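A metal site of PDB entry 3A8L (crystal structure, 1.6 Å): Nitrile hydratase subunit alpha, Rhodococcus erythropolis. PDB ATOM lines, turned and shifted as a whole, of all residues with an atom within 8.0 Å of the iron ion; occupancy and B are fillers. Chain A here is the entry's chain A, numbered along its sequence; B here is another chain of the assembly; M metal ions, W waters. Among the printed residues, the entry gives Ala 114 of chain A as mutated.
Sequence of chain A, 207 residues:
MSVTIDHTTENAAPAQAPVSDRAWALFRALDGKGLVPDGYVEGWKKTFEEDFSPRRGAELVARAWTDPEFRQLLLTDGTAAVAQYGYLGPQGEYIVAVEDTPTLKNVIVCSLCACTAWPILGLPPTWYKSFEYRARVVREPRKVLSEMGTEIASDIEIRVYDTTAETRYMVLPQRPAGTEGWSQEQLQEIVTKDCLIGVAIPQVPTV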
ATOM      1  N   GLN A  91      25.684 -29.422  35.401  1.00  0.00           N
ATOM      2  CA  GLN A  91      26.562 -28.433  34.772  1.00  0.00           C
ATOM      3  C   GLN A  91      27.905 -28.287  35.515  1.00  0.00           C
ATOM      4  O   GLN A  91      28.518 -27.225  35.544  1.00  0.00           O
ATOM      5  CB  GLN A  91      25.845 -27.092  34.614  1.00  0.00           C
ATOM      6  CG  GLN A  91      24.639 -27.158  33.692  1.00  0.00           C
ATOM      7  CD  GLN A  91      25.044 -27.555  32.282  1.00  0.00           C
ATOM      8  OE1 GLN A  91      25.874 -26.892  31.664  1.00  0.00           O
ATOM      9  NE2 GLN A  91      24.483 -28.649  31.790  1.00  0.00           N
ATOM     10  N   VAL A 109      34.274 -17.727  29.723  1.00  0.00           N
ATOM     11  CA  VAL A 109      33.025 -17.230  29.108  1.00  0.00           C
ATOM     12  C   VAL A 109      32.272 -18.395  28.470  1.00  0.00           C
ATOM     13  O   VAL A 109      32.842 -19.475  28.246  1.00  0.00           O
ATOM     14  CB  VAL A 109      33.335 -16.161  28.036  1.00  0.00           C
ATOM     15  CG1 VAL A 109      34.087 -16.752  26.841  1.00  0.00           C
ATOM     16  CG2 VAL A 109      32.040 -15.469  27.560  1.00  0.00           C
ATOM     17  N   CYS A 110      30.977 -18.193  28.193  1.00  0.00           N
ATOM     18  CA  CYS A 110      30.293 -19.046  27.221  1.00  0.00           C
ATOM     19  C   CYS A 110      29.769 -18.121  26.127  1.00  0.00           C
ATOM     20  O   CYS A 110      28.706 -17.487  26.267  1.00  0.00           O
ATOM     21  CB  CYS A 110      29.173 -19.836  27.875  1.00  0.00           C
ATOM     22  SG  CYS A 110      28.191 -20.796  26.713  1.00  0.00           S
ATOM     23  N   SER A 111      30.519 -17.987  25.028  1.00  0.00           N
ATOM     24  CA  SER A 111      30.116 -17.035  24.017  1.00  0.00           C
ATOM     25  C   SER A 111      28.790 -17.418  23.341  1.00  0.00           C
ATOM     26  O   SER A 111      28.086 -16.553  22.847  1.00  0.00           O
ATOM     27  CB  SER A 111      31.219 -16.833  22.968  1.00  0.00           C
ATOM     28  OG  SER A 111      31.338 -17.975  22.124  1.00  0.00           O
ATOM     29  N   LEU A 112      28.462 -18.716  23.332  1.00  0.00           N
ATOM     30  CA  LEU A 112      27.275 -19.210  22.629  1.00  0.00           C
ATOM     31  C   LEU A 112      26.001 -19.207  23.476  1.00  0.00           C
ATOM     32  O   LEU A 112      24.916 -19.347  22.928  1.00  0.00           O
ATOM     33  CB  LEU A 112      27.537 -20.623  22.099  1.00  0.00           C
ATOM     34  CG  LEU A 112      28.666 -20.723  21.080  1.00  0.00           C
ATOM     35  CD1 LEU A 112      28.971 -22.211  20.803  1.00  0.00           C
ATOM     36  CD2 LEU A 112      28.274 -20.026  19.785  1.00  0.00           C
ATOM     37  N   CSD A 113      26.135 -19.032  24.803  1.00  0.00           N
ATOM     38  CA  CSD A 113      24.983 -19.017  25.725  1.00  0.00           C
ATOM     39  CB  CSD A 113      24.165 -20.309  25.714  1.00  0.00           C
ATOM     40  SG  CSD A 113      25.251 -21.782  25.968  1.00  0.00           S
ATOM     41  C   CSD A 113      25.326 -18.557  27.128  1.00  0.00           C
ATOM     42  O   CSD A 113      25.294 -17.339  27.393  1.00  0.00           O
ATOM     43  OD1 CSD A 113      24.158 -22.942  26.109  1.00  0.00           O
ATOM     44  OD2 CSD A 113      26.059 -21.937  24.687  1.00  0.00           O
ATOM     45  N   ALA A 114      25.647 -19.466  28.059  1.00  0.00           N
ATOM     46  CA  ALA A 114      25.915 -19.036  29.447  1.00  0.00           C
ATOM     47  C   ALA A 114      26.643 -20.076  30.284  1.00  0.00           C
ATOM     48  O   ALA A 114      26.783 -19.952  31.510  1.00  0.00           O
ATOM     49  CB  ALA A 114      24.597 -18.646  30.141  1.00  0.00           C
ATOM     50  N   CSO A 115      27.083 -21.125  29.593  1.00  0.00           N
ATOM     51  CA  CSO A 115      27.687 -22.285  30.226  1.00  0.00           C
ATOM     52  CB  CSO A 115      28.314 -23.218  29.174  1.00  0.00           C
ATOM     53  SG  CSO A 115      27.127 -23.444  27.836  1.00  0.00           S
ATOM     54  C   CSO A 115      28.679 -21.886  31.325  1.00  0.00           C
ATOM     55  O   CSO A 115      29.568 -21.054  31.117  1.00  0.00           O
ATOM     56  OD  CSO A 115      26.036 -24.627  28.455  1.00  0.00           O
ATOM     57  N   THR A 116      28.463 -22.496  32.477  1.00  0.00           N
ATOM     58  CA  THR A 116      29.111 -22.147  33.740  1.00  0.00           C
ATOM     59  C   THR A 116      29.151 -23.393  34.634  1.00  0.00           C
ATOM     60  O   THR A 116      28.188 -24.164  34.639  1.00  0.00           O
ATOM     61  CB  THR A 116      28.241 -21.099  34.452  1.00  0.00           C
ATOM     62  OG1 THR A 116      28.291 -19.862  33.736  1.00  0.00           O
ATOM     63  CG2 THR A 116      28.661 -20.867  35.904  1.00  0.00           C
ATOM     64  N   TRP A 118      28.026 -24.525  37.389  1.00  0.00           N
ATOM     65  CA  TRP A 118      27.006 -24.158  38.408  1.00  0.00           C
ATOM     66  C   TRP A 118      27.318 -24.559  39.862  1.00  0.00           C
ATOM     67  O   TRP A 118      27.190 -23.726  40.749  1.00  0.00           O
ATOM     68  CB  TRP A 118      25.643 -24.748  38.064  1.00  0.00           C
ATOM     69  CG  TRP A 118      24.983 -24.200  36.845  1.00  0.00           C
ATOM     70  CD1 TRP A 118      25.355 -23.113  36.086  1.00  0.00           C
ATOM     71  CD2 TRP A 118      23.777 -24.702  36.256  1.00  0.00           C
ATOM     72  NE1 TRP A 118      24.451 -22.933  35.050  1.00  0.00           N
ATOM     73  CE2 TRP A 118      23.480 -23.890  35.138  1.00  0.00           C
ATOM     74  CE3 TRP A 118      22.909 -25.763  36.576  1.00  0.00           C
ATOM     75  CZ2 TRP A 118      22.351 -24.124  34.321  1.00  0.00           C
ATOM     76  CZ3 TRP A 118      21.795 -25.983  35.771  1.00  0.00           C
ATOM     77  CH2 TRP A 118      21.519 -25.162  34.660  1.00  0.00           C
ATOM     78  N   PRO A 124      25.150 -18.496  36.625  1.00  0.00           N
ATOM     79  CA  PRO A 124      25.785 -17.294  36.077  1.00  0.00           C
ATOM     80  C   PRO A 124      24.957 -16.037  36.366  1.00  0.00           C
ATOM     81  O   PRO A 124      23.735 -16.088  36.322  1.00  0.00           O
ATOM     82  CB  PRO A 124      25.811 -17.565  34.555  1.00  0.00           C
ATOM     83  CG  PRO A 124      24.768 -18.612  34.318  1.00  0.00           C
ATOM     84  CD  PRO A 124      24.764 -19.456  35.566  1.00  0.00           C
ATOM     85  N   TYR A 128      27.348 -11.916  32.988  1.00  0.00           N
ATOM     86  CA  TYR A 128      28.096 -12.968  32.311  1.00  0.00           C
ATOM     87  C   TYR A 128      27.326 -13.459  31.085  1.00  0.00           C
ATOM     88  O   TYR A 128      27.916 -13.888  30.079  1.00  0.00           O
ATOM     89  CB  TYR A 128      28.354 -14.087  33.294  1.00  0.00           C
ATOM     90  CG  TYR A 128      29.081 -15.308  32.777  1.00  0.00           C
ATOM     91  CD1 TYR A 128      28.367 -16.366  32.244  1.00  0.00           C
ATOM     92  CD2 TYR A 128      30.458 -15.416  32.896  1.00  0.00           C
ATOM     93  CE1 TYR A 128      29.029 -17.530  31.806  1.00  0.00           C
ATOM     94  CE2 TYR A 128      31.142 -16.556  32.474  1.00  0.00           C
ATOM     95  CZ  TYR A 128      30.416 -17.603  31.933  1.00  0.00           C
ATOM     96  OH  TYR A 128      31.077 -18.745  31.539  1.00  0.00           O
ATOM     97  N   LYS A 129      26.002 -13.437  31.202  1.00  0.00           N
ATOM     98  CA  LYS A 129      25.102 -13.829  30.124  1.00  0.00           C
ATOM     99  C   LYS A 129      24.875 -12.682  29.125  1.00  0.00           C
ATOM    100  O   LYS A 129      24.227 -12.894  28.098  1.00  0.00           O
ATOM    101  CB  LYS A 129      23.771 -14.293  30.731  1.00  0.00           C
ATOM    102  CG  LYS A 129      23.948 -15.460  31.683  1.00  0.00           C
ATOM    103  CD  LYS A 129      22.619 -15.930  32.277  1.00  0.00           C
ATOM    104  CE  LYS A 129      22.091 -14.994  33.347  1.00  0.00           C
ATOM    105  NZ  LYS A 129      20.882 -15.553  34.046  1.00  0.00           N
ATOM    106  N   ARG A 134      29.662 -11.735  26.202  1.00  0.00           N
ATOM    107  CA  ARG A 134      29.770 -12.814  25.223  1.00  0.00           C
ATOM    108  C   ARG A 134      30.475 -12.400  23.915  1.00  0.00           C
ATOM    109  O   ARG A 134      31.251 -13.181  23.342  1.00  0.00           O
ATOM    110  CB  ARG A 134      28.381 -13.399  24.946  1.00  0.00           C
ATOM    111  CG  ARG A 134      27.809 -14.156  26.147  1.00  0.00           C
ATOM    112  CD  ARG A 134      26.372 -14.639  25.910  1.00  0.00           C
ATOM    113  NE  ARG A 134      26.235 -15.275  24.603  1.00  0.00           N
ATOM    114  CZ  ARG A 134      25.088 -15.409  23.933  1.00  0.00           C
ATOM    115  NH1 ARG A 134      23.943 -14.978  24.460  1.00  0.00           N
ATOM    116  NH2 ARG A 134      25.099 -15.961  22.724  1.00  0.00           N
ATOM    117  N   ASP A 162      36.586 -20.465  26.269  1.00  0.00           N
ATOM    118  CA  ASP A 162      35.199 -20.399  25.795  1.00  0.00           C
ATOM    119  C   ASP A 162      34.550 -21.767  26.063  1.00  0.00           C
ATOM    120  O   ASP A 162      34.997 -22.822  25.555  1.00  0.00           O
ATOM    121  CB  ASP A 162      35.168 -20.028  24.306  1.00  0.00           C
ATOM    122  CG  ASP A 162      33.772 -19.576  23.842  1.00  0.00           C
ATOM    123  OD1 ASP A 162      32.795 -19.673  24.638  1.00  0.00           O
ATOM    124  OD2 ASP A 162      33.680 -19.116  22.668  1.00  0.00           O
ATOM    125  N   THR A 163      33.495 -21.751  26.881  1.00  0.00           N
ATOM    126  CA  THR A 163      32.867 -22.973  27.392  1.00  0.00           C
ATOM    127  C   THR A 163      31.868 -23.520  26.363  1.00  0.00           C
ATOM    128  O   THR A 163      30.651 -23.317  26.468  1.00  0.00           O
ATOM    129  CB  THR A 163      32.170 -22.718  28.756  1.00  0.00           C
ATOM    130  OG1 THR A 163      33.117 -22.116  29.655  1.00  0.00           O
ATOM    131  CG2 THR A 163      31.691 -24.025  29.376  1.00  0.00           C
ATOM    132  N   THR A 164      32.414 -24.219  25.365  1.00  0.00           N
ATOM    133  CA  THR A 164      31.652 -24.592  24.174  1.00  0.00           C
ATOM    134  C   THR A 164      31.153 -26.035  24.187  1.00  0.00           C
ATOM    135  O   THR A 164      30.377 -26.430  23.323  1.00  0.00           O
ATOM    136  CB  THR A 164      32.502 -24.378  22.897  1.00  0.00           C
ATOM    137  OG1 THR A 164      33.823 -24.921  23.103  1.00  0.00           O
ATOM    138  CG2 THR A 164      32.634 -22.894  22.602  1.00  0.00           C
ATOM    139  N   ALA A 165      31.624 -26.837  25.146  1.00  0.00           N
ATOM    140  CA  ALA A 165      31.196 -28.236  25.222  1.00  0.00           C
ATOM    141  C   ALA A 165      30.822 -28.613  26.641  1.00  0.00           C
ATOM    142  O   ALA A 165      30.018 -27.897  27.278  1.00  0.00           O
ATOM    143  CB  ALA A 165      32.238 -29.183  24.611  1.00  0.00           C
ATOM    144  N   ARG A 168      33.634 -27.901  32.316  1.00  0.00           N
ATOM    145  CA  ARG A 168      33.183 -26.757  33.101  1.00  0.00           C
ATOM    146  C   ARG A 168      34.369 -26.256  33.890  1.00  0.00           C
ATOM    147  O   ARG A 168      35.045 -27.026  34.588  1.00  0.00           O
ATOM    148  CB  ARG A 168      32.001 -27.145  33.981  1.00  0.00           C
ATOM    149  CG  ARG A 168      30.745 -27.507  33.177  1.00  0.00           C
ATOM    150  CD  ARG A 168      30.033 -26.277  32.623  1.00  0.00           C
ATOM    151  NE  ARG A 168      28.907 -26.655  31.771  1.00  0.00           N
ATOM    152  CZ  ARG A 168      29.002 -26.974  30.477  1.00  0.00           C
ATOM    153  NH1 ARG A 168      30.167 -26.914  29.836  1.00  0.00           N
ATOM    154  NH2 ARG A 168      27.911 -27.322  29.804  1.00  0.00           N
ATOM    155  N   TYR B  37      14.958 -23.401  34.182  1.00  0.00           N
ATOM    156  CA  TYR B  37      15.920 -24.496  34.428  1.00  0.00           C
ATOM    157  C   TYR B  37      15.224 -25.716  35.022  1.00  0.00           C
ATOM    158  O   TYR B  37      15.491 -26.859  34.625  1.00  0.00           O
ATOM    159  CB  TYR B  37      17.042 -24.074  35.369  1.00  0.00           C
ATOM    160  CG  TYR B  37      18.105 -23.155  34.782  1.00  0.00           C
ATOM    161  CD1 TYR B  37      18.285 -23.034  33.405  1.00  0.00           C
ATOM    162  CD2 TYR B  37      18.958 -22.431  35.637  1.00  0.00           C
ATOM    163  CE1 TYR B  37      19.278 -22.197  32.889  1.00  0.00           C
ATOM    164  CE2 TYR B  37      19.948 -21.603  35.125  1.00  0.00           C
ATOM    165  CZ  TYR B  37      20.101 -21.493  33.757  1.00  0.00           C
ATOM    166  OH  TYR B  37      21.103 -20.660  33.261  1.00  0.00           O
ATOM    167  N   ARG B  56      19.541 -25.891  23.840  1.00  0.00           N
ATOM    168  CA  ARG B  56      20.431 -24.883  23.259  1.00  0.00           C
ATOM    169  C   ARG B  56      19.994 -24.571  21.829  1.00  0.00           C
ATOM    170  O   ARG B  56      19.892 -23.405  21.422  1.00  0.00           O
ATOM    171  CB  ARG B  56      21.873 -25.353  23.262  1.00  0.00           C
ATOM    172  CG  ARG B  56      22.479 -25.534  24.639  1.00  0.00           C
ATOM    173  CD  ARG B  56      23.974 -25.684  24.552  1.00  0.00           C
ATOM    174  NE  ARG B  56      24.505 -25.850  25.890  1.00  0.00           N
ATOM    175  CZ  ARG B  56      24.712 -27.034  26.466  1.00  0.00           C
ATOM    176  NH1 ARG B  56      24.475 -28.155  25.760  1.00  0.00           N
ATOM    177  NH2 ARG B  56      25.189 -27.107  27.702  1.00  0.00           N
ATOM    178  N   TYR B  72      17.921 -13.545  28.967  1.00  0.00           N
ATOM    179  CA  TYR B  72      18.294 -14.951  28.994  1.00  0.00           C
ATOM    180  C   TYR B  72      17.198 -15.884  29.558  1.00  0.00           C
ATOM    181  O   TYR B  72      16.802 -16.826  28.887  1.00  0.00           O
ATOM    182  CB  TYR B  72      19.565 -15.125  29.839  1.00  0.00           C
ATOM    183  CG  TYR B  72      20.064 -16.549  29.859  1.00  0.00           C
ATOM    184  CD1 TYR B  72      20.929 -17.010  28.885  1.00  0.00           C
ATOM    185  CD2 TYR B  72      19.650 -17.431  30.850  1.00  0.00           C
ATOM    186  CE1 TYR B  72      21.373 -18.318  28.873  1.00  0.00           C
ATOM    187  CE2 TYR B  72      20.102 -18.744  30.858  1.00  0.00           C
ATOM    188  CZ  TYR B  72      20.952 -19.181  29.876  1.00  0.00           C
ATOM    189  OH  TYR B  72      21.398 -20.480  29.860  1.00  0.00           O
ATOM    190  N   TYR B  76      14.915 -19.006  27.618  1.00  0.00           N
ATOM    191  CA  TYR B  76      14.836 -20.385  28.071  1.00  0.00           C
ATOM    192  C   TYR B  76      13.378 -20.854  28.206  1.00  0.00           C
ATOM    193  O   TYR B  76      13.045 -21.954  27.747  1.00  0.00           O
ATOM    194  CB  TYR B  76      15.570 -20.528  29.413  1.00  0.00           C
ATOM    195  CG  TYR B  76      16.464 -21.743  29.489  1.00  0.00           C
ATOM    196  CD1 TYR B  76      17.773 -21.687  29.024  1.00  0.00           C
ATOM    197  CD2 TYR B  76      16.002 -22.928  30.037  1.00  0.00           C
ATOM    198  CE1 TYR B  76      18.597 -22.793  29.093  1.00  0.00           C
ATOM    199  CE2 TYR B  76      16.814 -24.047  30.118  1.00  0.00           C
ATOM    200  CZ  TYR B  76      18.119 -23.968  29.650  1.00  0.00           C
ATOM    201  OH  TYR B  76      18.947 -25.066  29.714  1.00  0.00           O
ATOM    202  N   ARG B 141      28.476 -26.921  18.021  1.00  0.00           N
ATOM    203  CA  ARG B 141      29.176 -26.268  19.137  1.00  0.00           C
ATOM    204  C   ARG B 141      30.559 -25.752  18.741  1.00  0.00           C
ATOM    205  O   ARG B 141      31.524 -25.884  19.486  1.00  0.00           O
ATOM    206  CB  ARG B 141      29.214 -27.202  20.343  1.00  0.00           C
ATOM    207  CG  ARG B 141      27.847 -27.474  20.920  1.00  0.00           C
ATOM    208  CD  ARG B 141      27.128 -26.187  21.338  1.00  0.00           C
ATOM    209  NE  ARG B 141      27.776 -25.586  22.505  1.00  0.00           N
ATOM    210  CZ  ARG B 141      27.355 -24.468  23.090  1.00  0.00           C
ATOM    211  NH1 ARG B 141      26.325 -23.828  22.571  1.00  0.00           N
ATOM    212  NH2 ARG B 141      27.938 -24.031  24.185  1.00  0.00           N
HETATM  213 FE    FE M   1      26.240 -21.439  27.807  1.00  0.00          FE
HETATM  214  O   HOH W   1      24.604 -22.036  28.784  1.00  0.00           O
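The guanidinium group (NH2) of Arg 141 of chain B sits close to SG of CSO 115, 3.8 Å away.
The guanidinium group (NH2) of Arg 56 of chain B lies within hydrogen-bond range of OD of CSO 115 (2.7 Å).
OH of Tyr 128 is in hydrogen-bond range of O of CSO 115, at 2.8 Å.
The backbone carbonyl oxygen of Ala 114 lies within hydrogen-bond range of the side-chain hydroxyl of Thr 116, 2.7 Å away.
OD2 of CSD 113 lies within salt-bridge range of NH1 of Arg 141 of chain B, 2.9 Å away.
The guanidinium group (NE) of Arg 56 of chain B is in salt-bridge range of OD1 of CSD 113.
The side-chain sulfur (SG) of Cys 110 sits close to the backbone carbonyl oxygen (O) of Thr 163 (3.5 Å).
N of Cys 110 lies within hydrogen-bond range of OH of Tyr 128 (3.4 Å).
Within 4 Å of the iron ion: Cys 110, CSD 113, Ala 114 and CSO 115.
The iron ion is bound by water W1, N of CSO 115, the backbone nitrogen of Ala 114, SG of CSD 113, SG of CSO 115 and the side-chain sulfur of Cys 110.
Water W1 lies within hydrogen-bond range of OD1 of CSD 113 (2.9 Å) and OD of CSO 115 (3.0 Å).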
